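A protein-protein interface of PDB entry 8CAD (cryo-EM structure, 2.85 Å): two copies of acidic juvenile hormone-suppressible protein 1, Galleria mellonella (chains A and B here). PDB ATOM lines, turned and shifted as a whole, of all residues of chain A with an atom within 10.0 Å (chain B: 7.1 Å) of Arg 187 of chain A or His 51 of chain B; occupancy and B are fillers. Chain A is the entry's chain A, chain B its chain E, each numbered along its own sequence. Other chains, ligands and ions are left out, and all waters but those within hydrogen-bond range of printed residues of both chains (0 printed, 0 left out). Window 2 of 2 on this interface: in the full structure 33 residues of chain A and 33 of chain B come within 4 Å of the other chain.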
ATOM      1  N   ARG A 180       8.816   4.613  21.861  1.00  0.00           N
ATOM      2  CA  ARG A 180      10.193   4.191  22.096  1.00  0.00           C
ATOM      3  C   ARG A 180      11.002   4.195  20.801  1.00  0.00           C
ATOM      4  O   ARG A 180      12.121   4.720  20.756  1.00  0.00           O
ATOM      5  CB  ARG A 180      10.210   2.810  22.754  1.00  0.00           C
ATOM      6  CG  ARG A 180       9.681   2.814  24.174  1.00  0.00           C
ATOM      7  CD  ARG A 180       9.718   1.435  24.802  1.00  0.00           C
ATOM      8  NE  ARG A 180       9.164   1.436  26.152  1.00  0.00           N
ATOM      9  CZ  ARG A 180       8.959   0.348  26.881  1.00  0.00           C
ATOM     10  NH1 ARG A 180       9.244  -0.859  26.419  1.00  0.00           N
ATOM     11  NH2 ARG A 180       8.452   0.475  28.104  1.00  0.00           N
ATOM     12  N   ILE A 181      10.455   3.607  19.733  1.00  0.00           N
ATOM     13  CA  ILE A 181      11.194   3.535  18.473  1.00  0.00           C
ATOM     14  C   ILE A 181      11.447   4.929  17.922  1.00  0.00           C
ATOM     15  O   ILE A 181      12.484   5.179  17.296  1.00  0.00           O
ATOM     16  CB  ILE A 181      10.453   2.648  17.443  1.00  0.00           C
ATOM     17  CG1 ILE A 181       9.091   3.251  17.076  1.00  0.00           C
ATOM     18  CG2 ILE A 181      10.319   1.219  17.975  1.00  0.00           C
ATOM     19  CD1 ILE A 181       8.362   2.536  15.949  1.00  0.00           C
ATOM     20  N   THR A 182      10.510   5.855  18.131  1.00  0.00           N
ATOM     21  CA  THR A 182      10.699   7.214  17.633  1.00  0.00           C
ATOM     22  C   THR A 182      11.770   7.947  18.433  1.00  0.00           C
ATOM     23  O   THR A 182      12.701   8.526  17.862  1.00  0.00           O
ATOM     24  CB  THR A 182       9.374   7.981  17.681  1.00  0.00           C
ATOM     25  OG1 THR A 182       8.389   7.278  16.913  1.00  0.00           O
ATOM     26  CG2 THR A 182       9.549   9.382  17.116  1.00  0.00           C
ATOM     27  N   THR A 183      11.651   7.934  19.763  1.00  0.00           N
ATOM     28  CA  THR A 183      12.589   8.685  20.594  1.00  0.00           C
ATOM     29  C   THR A 183      13.983   8.063  20.560  1.00  0.00           C
ATOM     30  O   THR A 183      14.978   8.741  20.841  1.00  0.00           O
ATOM     31  CB  THR A 183      12.071   8.767  22.027  1.00  0.00           C
ATOM     32  OG1 THR A 183      11.990   7.453  22.588  1.00  0.00           O
ATOM     33  CG2 THR A 183      10.698   9.424  22.052  1.00  0.00           C
ATOM     34  N   HIS A 184      14.077   6.774  20.234  1.00  0.00           N
ATOM     35  CA  HIS A 184      15.369   6.099  20.191  1.00  0.00           C
ATOM     36  C   HIS A 184      16.205   6.547  18.998  1.00  0.00           C
ATOM     37  O   HIS A 184      17.398   6.237  18.920  1.00  0.00           O
ATOM     38  CB  HIS A 184      15.177   4.582  20.164  1.00  0.00           C
ATOM     39  CG  HIS A 184      15.255   3.951  21.522  1.00  0.00           C
ATOM     40  ND1 HIS A 184      16.316   4.172  22.372  1.00  0.00           N
ATOM     41  CD2 HIS A 184      14.411   3.120  22.181  1.00  0.00           C
ATOM     42  CE1 HIS A 184      16.128   3.503  23.495  1.00  0.00           C
ATOM     43  NE2 HIS A 184      14.980   2.853  23.406  1.00  0.00           N
ATOM     44  N   GLY A 185      15.603   7.295  18.080  1.00  0.00           N
ATOM     45  CA  GLY A 185      16.300   7.665  16.865  1.00  0.00           C
ATOM     46  C   GLY A 185      16.491   6.512  15.906  1.00  0.00           C
ATOM     47  O   GLY A 185      17.371   6.568  15.038  1.00  0.00           O
ATOM     48  N   GLN A 186      15.678   5.463  16.034  1.00  0.00           N
ATOM     49  CA  GLN A 186      15.757   4.285  15.173  1.00  0.00           C
ATOM     50  C   GLN A 186      17.130   3.620  15.240  1.00  0.00           C
ATOM     51  O   GLN A 186      17.607   3.057  14.251  1.00  0.00           O
ATOM     52  CB  GLN A 186      15.403   4.630  13.722  1.00  0.00           C
ATOM     53  CG  GLN A 186      13.939   4.996  13.502  1.00  0.00           C
ATOM     54  CD  GLN A 186      13.547   6.306  14.160  1.00  0.00           C
ATOM     55  OE1 GLN A 186      12.560   6.373  14.892  1.00  0.00           O
ATOM     56  NE2 GLN A 186      14.314   7.356  13.894  1.00  0.00           N
ATOM     57  N   ARG A 187      17.778   3.678  16.401  1.00  0.00           N
ATOM     58  CA  ARG A 187      19.000   2.921  16.652  1.00  0.00           C
ATOM     59  C   ARG A 187      18.743   1.626  17.399  1.00  0.00           C
ATOM     60  O   ARG A 187      19.310   0.592  17.043  1.00  0.00           O
ATOM     61  CB  ARG A 187      20.004   3.764  17.447  1.00  0.00           C
ATOM     62  CG  ARG A 187      21.410   3.166  17.492  1.00  0.00           C
ATOM     63  CD  ARG A 187      21.627   2.250  18.698  1.00  0.00           C
ATOM     64  NE  ARG A 187      21.493   2.965  19.962  1.00  0.00           N
ATOM     65  CZ  ARG A 187      21.517   2.390  21.157  1.00  0.00           C
ATOM     66  NH1 ARG A 187      21.660   1.082  21.296  1.00  0.00           N
ATOM     67  NH2 ARG A 187      21.390   3.148  22.243  1.00  0.00           N
ATOM     68  N   MET A 188      17.915   1.657  18.444  1.00  0.00           N
ATOM     69  CA  MET A 188      17.443   0.429  19.066  1.00  0.00           C
ATOM     70  C   MET A 188      16.232  -0.148  18.350  1.00  0.00           C
ATOM     71  O   MET A 188      15.774  -1.237  18.716  1.00  0.00           O
ATOM     72  CB  MET A 188      17.108   0.668  20.540  1.00  0.00           C
ATOM     73  CG  MET A 188      18.336   0.846  21.427  1.00  0.00           C
ATOM     74  SD  MET A 188      17.971   0.960  23.188  1.00  0.00           S
ATOM     75  CE  MET A 188      16.951  -0.485  23.429  1.00  0.00           C
ATOM     76  N   LEU A 189      15.695   0.562  17.354  1.00  0.00           N
ATOM     77  CA  LEU A 189      14.622   0.006  16.540  1.00  0.00           C
ATOM     78  C   LEU A 189      15.096  -1.227  15.780  1.00  0.00           C
ATOM     79  O   LEU A 189      14.379  -2.230  15.700  1.00  0.00           O
ATOM     80  CB  LEU A 189      14.102   1.074  15.577  1.00  0.00           C
ATOM     81  CG  LEU A 189      12.989   0.686  14.597  1.00  0.00           C
ATOM     82  CD1 LEU A 189      12.106   1.890  14.275  1.00  0.00           C
ATOM     83  CD2 LEU A 189      13.566   0.101  13.310  1.00  0.00           C
ATOM     84  N   GLU A 190      16.304  -1.173  15.214  1.00  0.00           N
ATOM     85  CA  GLU A 190      16.841  -2.331  14.510  1.00  0.00           C
ATOM     86  C   GLU A 190      17.124  -3.495  15.448  1.00  0.00           C
ATOM     87  O   GLU A 190      17.285  -4.626  14.974  1.00  0.00           O
ATOM     88  CB  GLU A 190      18.112  -1.938  13.746  1.00  0.00           C
ATOM     89  CG  GLU A 190      19.246  -1.407  14.615  1.00  0.00           C
ATOM     90  CD  GLU A 190      20.151  -2.501  15.153  1.00  0.00           C
ATOM     91  OE1 GLU A 190      19.978  -3.674  14.760  1.00  0.00           O
ATOM     92  OE2 GLU A 190      21.041  -2.184  15.970  1.00  0.00           O
ATOM     93  N   HIS A 191      17.189  -3.250  16.758  1.00  0.00           N
ATOM     94  CA  HIS A 191      17.228  -4.351  17.713  1.00  0.00           C
ATOM     95  C   HIS A 191      15.867  -5.028  17.811  1.00  0.00           C
ATOM     96  O   HIS A 191      15.786  -6.254  17.961  1.00  0.00           O
ATOM     97  CB  HIS A 191      17.683  -3.839  19.080  1.00  0.00           C
ATOM     98  CG  HIS A 191      17.879  -4.919  20.098  1.00  0.00           C
ATOM     99  ND1 HIS A 191      16.844  -5.421  20.858  1.00  0.00           N
ATOM    100  CD2 HIS A 191      18.990  -5.589  20.486  1.00  0.00           C
ATOM    101  CE1 HIS A 191      17.308  -6.355  21.668  1.00  0.00           C
ATOM    102  NE2 HIS A 191      18.607  -6.476  21.463  1.00  0.00           N
ATOM    103  N   TYR A 192      14.791  -4.252  17.730  1.00  0.00           N
ATOM    104  CA  TYR A 192      13.449  -4.817  17.675  1.00  0.00           C
ATOM    105  C   TYR A 192      13.291  -5.643  16.402  1.00  0.00           C
ATOM    106  O   TYR A 192      13.521  -5.117  15.302  1.00  0.00           O
ATOM    107  CB  TYR A 192      12.389  -3.715  17.702  1.00  0.00           C
ATOM    108  CG  TYR A 192      12.231  -3.010  19.030  1.00  0.00           C
ATOM    109  CD1 TYR A 192      12.104  -3.725  20.212  1.00  0.00           C
ATOM    110  CD2 TYR A 192      12.200  -1.623  19.099  1.00  0.00           C
ATOM    111  CE1 TYR A 192      11.953  -3.081  21.425  1.00  0.00           C
ATOM    112  CE2 TYR A 192      12.050  -0.970  20.307  1.00  0.00           C
ATOM    113  CZ  TYR A 192      11.928  -1.703  21.466  1.00  0.00           C
ATOM    114  OH  TYR A 192      11.778  -1.057  22.671  1.00  0.00           O
ATOM    115  N   PRO A 193      12.909  -6.920  16.492  1.00  0.00           N
ATOM    116  CA  PRO A 193      12.636  -7.666  15.255  1.00  0.00           C
ATOM    117  C   PRO A 193      11.267  -7.365  14.673  1.00  0.00           C
ATOM    118  O   PRO A 193      11.077  -7.480  13.455  1.00  0.00           O
ATOM    119  CB  PRO A 193      12.768  -9.129  15.700  1.00  0.00           C
ATOM    120  CG  PRO A 193      12.388  -9.112  17.139  1.00  0.00           C
ATOM    121  CD  PRO A 193      12.843  -7.784  17.685  1.00  0.00           C
ATOM    122  N   THR A 195       9.570  -4.474  14.344  1.00  0.00           N
ATOM    123  CA  THR A 195       9.548  -3.312  13.469  1.00  0.00           C
ATOM    124  C   THR A 195      10.459  -3.524  12.261  1.00  0.00           C
ATOM    125  O   THR A 195      11.439  -4.274  12.308  1.00  0.00           O
ATOM    126  CB  THR A 195       9.976  -2.061  14.236  1.00  0.00           C
ATOM    127  OG1 THR A 195      11.300  -2.241  14.751  1.00  0.00           O
ATOM    128  CG2 THR A 195       9.020  -1.792  15.392  1.00  0.00           C
ATOM    129  N   VAL A 197      11.546  -1.453   8.151  1.00  0.00           N
ATOM    130  CA  VAL A 197      11.505  -0.268   7.300  1.00  0.00           C
ATOM    131  C   VAL A 197      11.006  -0.710   5.929  1.00  0.00           C
ATOM    132  O   VAL A 197      11.757  -1.281   5.132  1.00  0.00           O
ATOM    133  CB  VAL A 197      12.873   0.414   7.212  1.00  0.00           C
ATOM    134  CG1 VAL A 197      12.792   1.658   6.336  1.00  0.00           C
ATOM    135  CG2 VAL A 197      13.382   0.768   8.602  1.00  0.00           C
ATOM    136  N   VAL A 203       8.572   3.573   9.147  1.00  0.00           N
ATOM    137  CA  VAL A 203       8.898   2.345   9.861  1.00  0.00           C
ATOM    138  C   VAL A 203       7.596   1.680  10.285  1.00  0.00           C
ATOM    139  O   VAL A 203       6.702   2.336  10.832  1.00  0.00           O
ATOM    140  CB  VAL A 203       9.806   2.613  11.078  1.00  0.00           C
ATOM    141  CG1 VAL A 203       9.113   3.522  12.082  1.00  0.00           C
ATOM    142  CG2 VAL A 203      10.216   1.301  11.724  1.00  0.00           C
ATOM    143  N   LYS A 496       9.890  11.267  12.380  1.00  0.00           N
ATOM    144  CA  LYS A 496       9.678  10.091  11.545  1.00  0.00           C
ATOM    145  C   LYS A 496       8.194   9.780  11.400  1.00  0.00           C
ATOM    146  O   LYS A 496       7.342  10.510  11.909  1.00  0.00           O
ATOM    147  CB  LYS A 496      10.408   8.879  12.130  1.00  0.00           C
ATOM    148  CG  LYS A 496      11.929   8.985  12.107  1.00  0.00           C
ATOM    149  CD  LYS A 496      12.478   9.247  10.707  1.00  0.00           C
ATOM    150  CE  LYS A 496      11.931   8.266   9.679  1.00  0.00           C
ATOM    151  NZ  LYS A 496      12.109   6.848  10.097  1.00  0.00           N
ATOM    152  N   PHE B  44      22.474  -1.145  34.824  1.00  0.00           N
ATOM    153  CA  PHE B  44      22.263   0.203  34.304  1.00  0.00           C
ATOM    154  C   PHE B  44      21.023   0.308  33.423  1.00  0.00           C
ATOM    155  O   PHE B  44      20.273   1.284  33.534  1.00  0.00           O
ATOM    156  CB  PHE B  44      23.494   0.668  33.515  1.00  0.00           C
ATOM    157  CG  PHE B  44      24.630   1.170  34.377  1.00  0.00           C
ATOM    158  CD1 PHE B  44      24.550   1.149  35.762  1.00  0.00           C
ATOM    159  CD2 PHE B  44      25.778   1.677  33.790  1.00  0.00           C
ATOM    160  CE1 PHE B  44      25.592   1.615  36.539  1.00  0.00           C
ATOM    161  CE2 PHE B  44      26.824   2.145  34.565  1.00  0.00           C
ATOM    162  CZ  PHE B  44      26.730   2.113  35.941  1.00  0.00           C
ATOM    163  N   HIS B  45      20.786  -0.667  32.547  1.00  0.00           N
ATOM    164  CA  HIS B  45      19.626  -0.637  31.656  1.00  0.00           C
ATOM    165  C   HIS B  45      19.216  -2.065  31.338  1.00  0.00           C
ATOM    166  O   HIS B  45      19.652  -2.645  30.335  1.00  0.00           O
ATOM    167  CB  HIS B  45      19.919   0.142  30.376  1.00  0.00           C
ATOM    168  CG  HIS B  45      19.828   1.627  30.541  1.00  0.00           C
ATOM    169  ND1 HIS B  45      18.641   2.317  30.418  1.00  0.00           N
ATOM    170  CD2 HIS B  45      20.774   2.554  30.820  1.00  0.00           C
ATOM    171  CE1 HIS B  45      18.860   3.605  30.614  1.00  0.00           C
ATOM    172  NE2 HIS B  45      20.146   3.775  30.859  1.00  0.00           N
ATOM    173  N   GLU B  48      17.057  -2.428  27.880  1.00  0.00           N
ATOM    174  CA  GLU B  48      17.882  -2.139  26.719  1.00  0.00           C
ATOM    175  C   GLU B  48      19.065  -3.105  26.650  1.00  0.00           C
ATOM    176  O   GLU B  48      19.491  -3.648  27.672  1.00  0.00           O
ATOM    177  CB  GLU B  48      18.396  -0.707  26.780  1.00  0.00           C
ATOM    178  CG  GLU B  48      17.308   0.336  26.964  1.00  0.00           C
ATOM    179  CD  GLU B  48      17.865   1.711  27.272  1.00  0.00           C
ATOM    180  OE1 GLU B  48      18.982   2.023  26.809  1.00  0.00           O
ATOM    181  OE2 GLU B  48      17.190   2.481  27.990  1.00  0.00           O
ATOM    182  N   PRO B  49      19.617  -3.337  25.453  1.00  0.00           N
ATOM    183  CA  PRO B  49      20.707  -4.313  25.324  1.00  0.00           C
ATOM    184  C   PRO B  49      22.041  -3.789  25.834  1.00  0.00           C
ATOM    185  O   PRO B  49      22.125  -2.663  26.334  1.00  0.00           O
ATOM    186  CB  PRO B  49      20.746  -4.585  23.815  1.00  0.00           C
ATOM    187  CG  PRO B  49      20.290  -3.311  23.207  1.00  0.00           C
ATOM    188  CD  PRO B  49      19.244  -2.761  24.148  1.00  0.00           C
ATOM    189  N   ILE B  50      23.094  -4.597  25.703  1.00  0.00           N
ATOM    190  CA  ILE B  50      24.407  -4.206  26.199  1.00  0.00           C
ATOM    191  C   ILE B  50      24.977  -3.106  25.316  1.00  0.00           C
ATOM    192  O   ILE B  50      25.031  -3.237  24.085  1.00  0.00           O
ATOM    193  CB  ILE B  50      25.352  -5.417  26.250  1.00  0.00           C
ATOM    194  CG1 ILE B  50      24.891  -6.425  27.304  1.00  0.00           C
ATOM    195  CG2 ILE B  50      26.772  -4.968  26.561  1.00  0.00           C
ATOM    196  CD1 ILE B  50      25.159  -5.986  28.730  1.00  0.00           C
ATOM    197  N   HIS B  51      25.413  -2.014  25.944  1.00  0.00           N
ATOM    198  CA  HIS B  51      26.009  -0.891  25.234  1.00  0.00           C
ATOM    199  C   HIS B  51      27.522  -0.825  25.384  1.00  0.00           C
ATOM    200  O   HIS B  51      28.187  -0.229  24.530  1.00  0.00           O
ATOM    201  CB  HIS B  51      25.403   0.428  25.730  1.00  0.00           C
ATOM    202  CG  HIS B  51      23.907   0.452  25.705  1.00  0.00           C
ATOM    203  ND1 HIS B  51      23.167  -0.199  24.742  1.00  0.00           N
ATOM    204  CD2 HIS B  51      23.011   1.046  26.529  1.00  0.00           C
ATOM    205  CE1 HIS B  51      21.881  -0.005  24.972  1.00  0.00           C
ATOM    206  NE2 HIS B  51      21.759   0.746  26.051  1.00  0.00           N
ATOM    207  N   ILE B  52      28.074  -1.416  26.438  1.00  0.00           N
ATOM    208  CA  ILE B  52      29.511  -1.370  26.683  1.00  0.00           C
ATOM    209  C   ILE B  52      30.191  -2.445  25.843  1.00  0.00           C
ATOM    210  O   ILE B  52      29.761  -3.605  25.829  1.00  0.00           O
ATOM    211  CB  ILE B  52      29.809  -1.547  28.180  1.00  0.00           C
ATOM    212  CG1 ILE B  52      29.159  -0.413  28.979  1.00  0.00           C
ATOM    213  CG2 ILE B  52      31.303  -1.581  28.413  1.00  0.00           C
ATOM    214  CD1 ILE B  52      29.226  -0.591  30.483  1.00  0.00           C
ATOM    215  N   LYS B  53      31.266  -2.062  25.151  1.00  0.00           N
ATOM    216  CA  LYS B  53      31.817  -2.908  24.096  1.00  0.00           C
ATOM    217  C   LYS B  53      32.450  -4.180  24.654  1.00  0.00           C
ATOM    218  O   LYS B  53      32.200  -5.279  24.147  1.00  0.00           O
ATOM    219  CB  LYS B  53      32.834  -2.115  23.275  1.00  0.00           C
ATOM    220  CG  LYS B  53      32.241  -0.897  22.580  1.00  0.00           C
ATOM    221  CD  LYS B  53      33.247  -0.220  21.664  1.00  0.00           C
ATOM    222  CE  LYS B  53      32.612   0.936  20.906  1.00  0.00           C
ATOM    223  NZ  LYS B  53      33.532   1.525  19.894  1.00  0.00           N
ATOM    224  N   GLU B  54      33.289  -4.055  25.688  1.00  0.00           N
ATOM    225  CA  GLU B  54      34.000  -5.234  26.175  1.00  0.00           C
ATOM    226  C   GLU B  54      33.040  -6.273  26.743  1.00  0.00           C
ATOM    227  O   GLU B  54      33.318  -7.476  26.672  1.00  0.00           O
ATOM    228  CB  GLU B  54      35.051  -4.843  27.220  1.00  0.00           C
ATOM    229  CG  GLU B  54      34.512  -4.284  28.529  1.00  0.00           C
ATOM    230  CD  GLU B  54      34.184  -2.810  28.443  1.00  0.00           C
ATOM    231  OE1 GLU B  54      34.096  -2.281  27.314  1.00  0.00           O
ATOM    232  OE2 GLU B  54      34.012  -2.175  29.506  1.00  0.00           O
ATOM    233  N   GLN B  55      31.906  -5.840  27.293  1.00  0.00           N
ATOM    234  CA  GLN B  55      30.899  -6.802  27.728  1.00  0.00           C
ATOM    235  C   GLN B  55      30.304  -7.545  26.537  1.00  0.00           C
ATOM    236  O   GLN B  55      30.029  -8.747  26.623  1.00  0.00           O
ATOM    237  CB  GLN B  55      29.811  -6.096  28.535  1.00  0.00           C
ATOM    238  CG  GLN B  55      30.257  -5.700  29.935  1.00  0.00           C
ATOM    239  CD  GLN B  55      29.159  -5.033  30.735  1.00  0.00           C
ATOM    240  OE1 GLN B  55      28.055  -4.820  30.239  1.00  0.00           O
ATOM    241  NE2 GLN B  55      29.458  -4.701  31.986  1.00  0.00           N
ATOM    242  N   GLN B  56      30.112  -6.849  25.414  1.00  0.00           N
ATOM    243  CA  GLN B  56      29.686  -7.528  24.193  1.00  0.00           C
ATOM    244  C   GLN B  56      30.731  -8.541  23.748  1.00  0.00           C
ATOM    245  O   GLN B  56      30.393  -9.652  23.320  1.00  0.00           O
ATOM    246  CB  GLN B  56      29.432  -6.508  23.082  1.00  0.00           C
ATOM    247  CG  GLN B  56      28.450  -5.409  23.446  1.00  0.00           C
ATOM    248  CD  GLN B  56      28.452  -4.272  22.444  1.00  0.00           C
ATOM    249  OE1 GLN B  56      28.904  -4.429  21.310  1.00  0.00           O
ATOM    250  NE2 GLN B  56      27.953  -3.114  22.861  1.00  0.00           N
ATOM    251  N   ARG B 131      23.120 -11.983  31.268  1.00  0.00           N
ATOM    252  CA  ARG B 131      22.544 -10.675  30.974  1.00  0.00           C
ATOM    253  C   ARG B 131      22.269 -10.534  29.488  1.00  0.00           C
ATOM    254  O   ARG B 131      21.260  -9.940  29.091  1.00  0.00           O
ATOM    255  CB  ARG B 131      23.497  -9.571  31.446  1.00  0.00           C
ATOM    256  CG  ARG B 131      23.195  -8.170  30.908  1.00  0.00           C
ATOM    257  CD  ARG B 131      21.872  -7.622  31.416  1.00  0.00           C
ATOM    258  NE  ARG B 131      21.455  -6.441  30.667  1.00  0.00           N
ATOM    259  CZ  ARG B 131      21.886  -5.209  30.903  1.00  0.00           C
ATOM    260  NH1 ARG B 131      22.757  -4.950  31.865  1.00  0.00           N
ATOM    261  NH2 ARG B 131      21.434  -4.210  30.150  1.00  0.00           N
ATOM    262  N   LEU B 484      16.856   6.690  27.200  1.00  0.00           N
ATOM    263  CA  LEU B 484      17.680   7.792  26.725  1.00  0.00           C
ATOM    264  C   LEU B 484      18.330   7.433  25.394  1.00  0.00           C
ATOM    265  O   LEU B 484      18.793   6.306  25.196  1.00  0.00           O
ATOM    266  CB  LEU B 484      18.753   8.130  27.762  1.00  0.00           C
ATOM    267  CG  LEU B 484      19.742   9.233  27.378  1.00  0.00           C
ATOM    268  CD1 LEU B 484      19.001  10.511  27.028  1.00  0.00           C
ATOM    269  CD2 LEU B 484      20.741   9.486  28.500  1.00  0.00           C
ATOM    270  N   ASN B 485      18.355   8.398  24.480  1.00  0.00           N
ATOM    271  CA  ASN B 485      18.986   8.239  23.178  1.00  0.00           C
ATOM    272  C   ASN B 485      20.249   9.089  23.128  1.00  0.00           C
ATOM    273  O   ASN B 485      20.217  10.276  23.470  1.00  0.00           O
ATOM    274  CB  ASN B 485      18.028   8.638  22.055  1.00  0.00           C
ATOM    275  CG  ASN B 485      18.644   8.484  20.678  1.00  0.00           C
ATOM    276  OD1 ASN B 485      19.668   7.820  20.515  1.00  0.00           O
ATOM    277  ND2 ASN B 485      18.020   9.099  19.678  1.00  0.00           N
ATOM    278  N   GLU B 486      21.352   8.481  22.700  1.00  0.00           N
ATOM    279  CA  GLU B 486      22.647   9.155  22.667  1.00  0.00           C
ATOM    280  C   GLU B 486      23.014   9.693  24.046  1.00  0.00           C
ATOM    281  O   GLU B 486      23.015  10.903  24.271  1.00  0.00           O
ATOM    282  CB  GLU B 486      22.642  10.295  21.643  1.00  0.00           C
ATOM    283  CG  GLU B 486      22.618   9.830  20.196  1.00  0.00           C
ATOM    284  CD  GLU B 486      22.785  10.975  19.215  1.00  0.00           C
ATOM    285  OE1 GLU B 486      22.770  12.143  19.655  1.00  0.00           O
ATOM    286  OE2 GLU B 486      22.932  10.705  18.004  1.00  0.00           O
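O of Thr 183 of chain A sits at hydrogen-bond distance from ND2 of Asn 485 of chain B (3.3 Å). ND2 of Asn 485 of chain B lies within hydrogen-bond range of O of His 184 of chain A (3.0 Å). N of Gly 185 of chain A lies close to ND2 of Asn 485 of chain B, at 3.4 Å.
A ring nitrogen (NE2) of His 184 of chain A sits close to the side-chain sulfur (SD) of Met 188 of chain A, 3.5 Å away. The side-chain carboxylate (OE2) of Glu 48 of chain B lies within hydrogen-bond range of a ring nitrogen (ND1) of His 45 of chain B, 2.8 Å away. OE1 of Glu 48 of chain B is in hydrogen-bond range of NE2 of His 51 of chain B (3.1 Å). NH2 of Arg 131 of chain B lies within hydrogen-bond range of O of Glu 48 of chain B, at 3.2 Å. The backbone carbonyl oxygen of Pro 49 of chain B sits close to a ring nitrogen (ND1) of His 51 of chain B, at 3.1 Å. The side-chain amide nitrogen (NE2) of Gln 56 of chain B is in hydrogen-bond range of the backbone carbonyl oxygen (O) of His 51 of chain B, 3.3 Å away.
Arg 187 of chain A touches His 51 of chain B (NH1 to CE1, 3.8 Å). CG of Glu 48 of chain B touches CE of Met 188 of chain A, 3.6 Å away. Met 188 of chain A touches Pro 49 of chain B. NE2 of His 191 of chain A touches CB of Pro 49 of chain B (3.7 Å).
Printed residues of chain B within 4 Å of Arg 187 of chain A: His 51 (3.8 Å). Of the printed residues of chain A, His 51 of chain B touches Arg 187. Ile 50 of chain B touches none of the printed residues of chain A. No residue of chain A comes within 4 Å of Ile 52 of chain B. Printed residues of chain A within 4 Å of Glu 48 of chain B: Met 188. Printed residues of chain B within 4 Å of His 191 of chain A: Pro 49 (3.7 Å). The nearest residue of chain A that does not touch His 51 of chain B is Met 188 of chain A (4.4 Å). The nearest printed residue of chain B that does not touch His 191 of chain A is Glu 48 of chain B (6.2 Å).
Of the 18 printed residues of chain A, 6 touch a printed residue of chain B. Printed residues of chain A that touch a printed residue of chain B: Thr 183, His 184, Gly 185, Arg 187, Met 188 and His 191. Hydrophobic or aromatic side chains of chain A within 4 Å of the printed part of chain B: Met 188 and His 191. Of the 15 printed residues of chain B, 4 touch a printed residue of chain A. Along chain B the printed residues that touch a printed residue of chain A span positions 48 to 485. Among the printed residues, 7 pairs touch across the chains. Among the printed residues, no Asp or Glu carboxylate lies within 4 Å of a Lys or Arg side-chain nitrogen of the other chain.
No position is printed for both chains.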
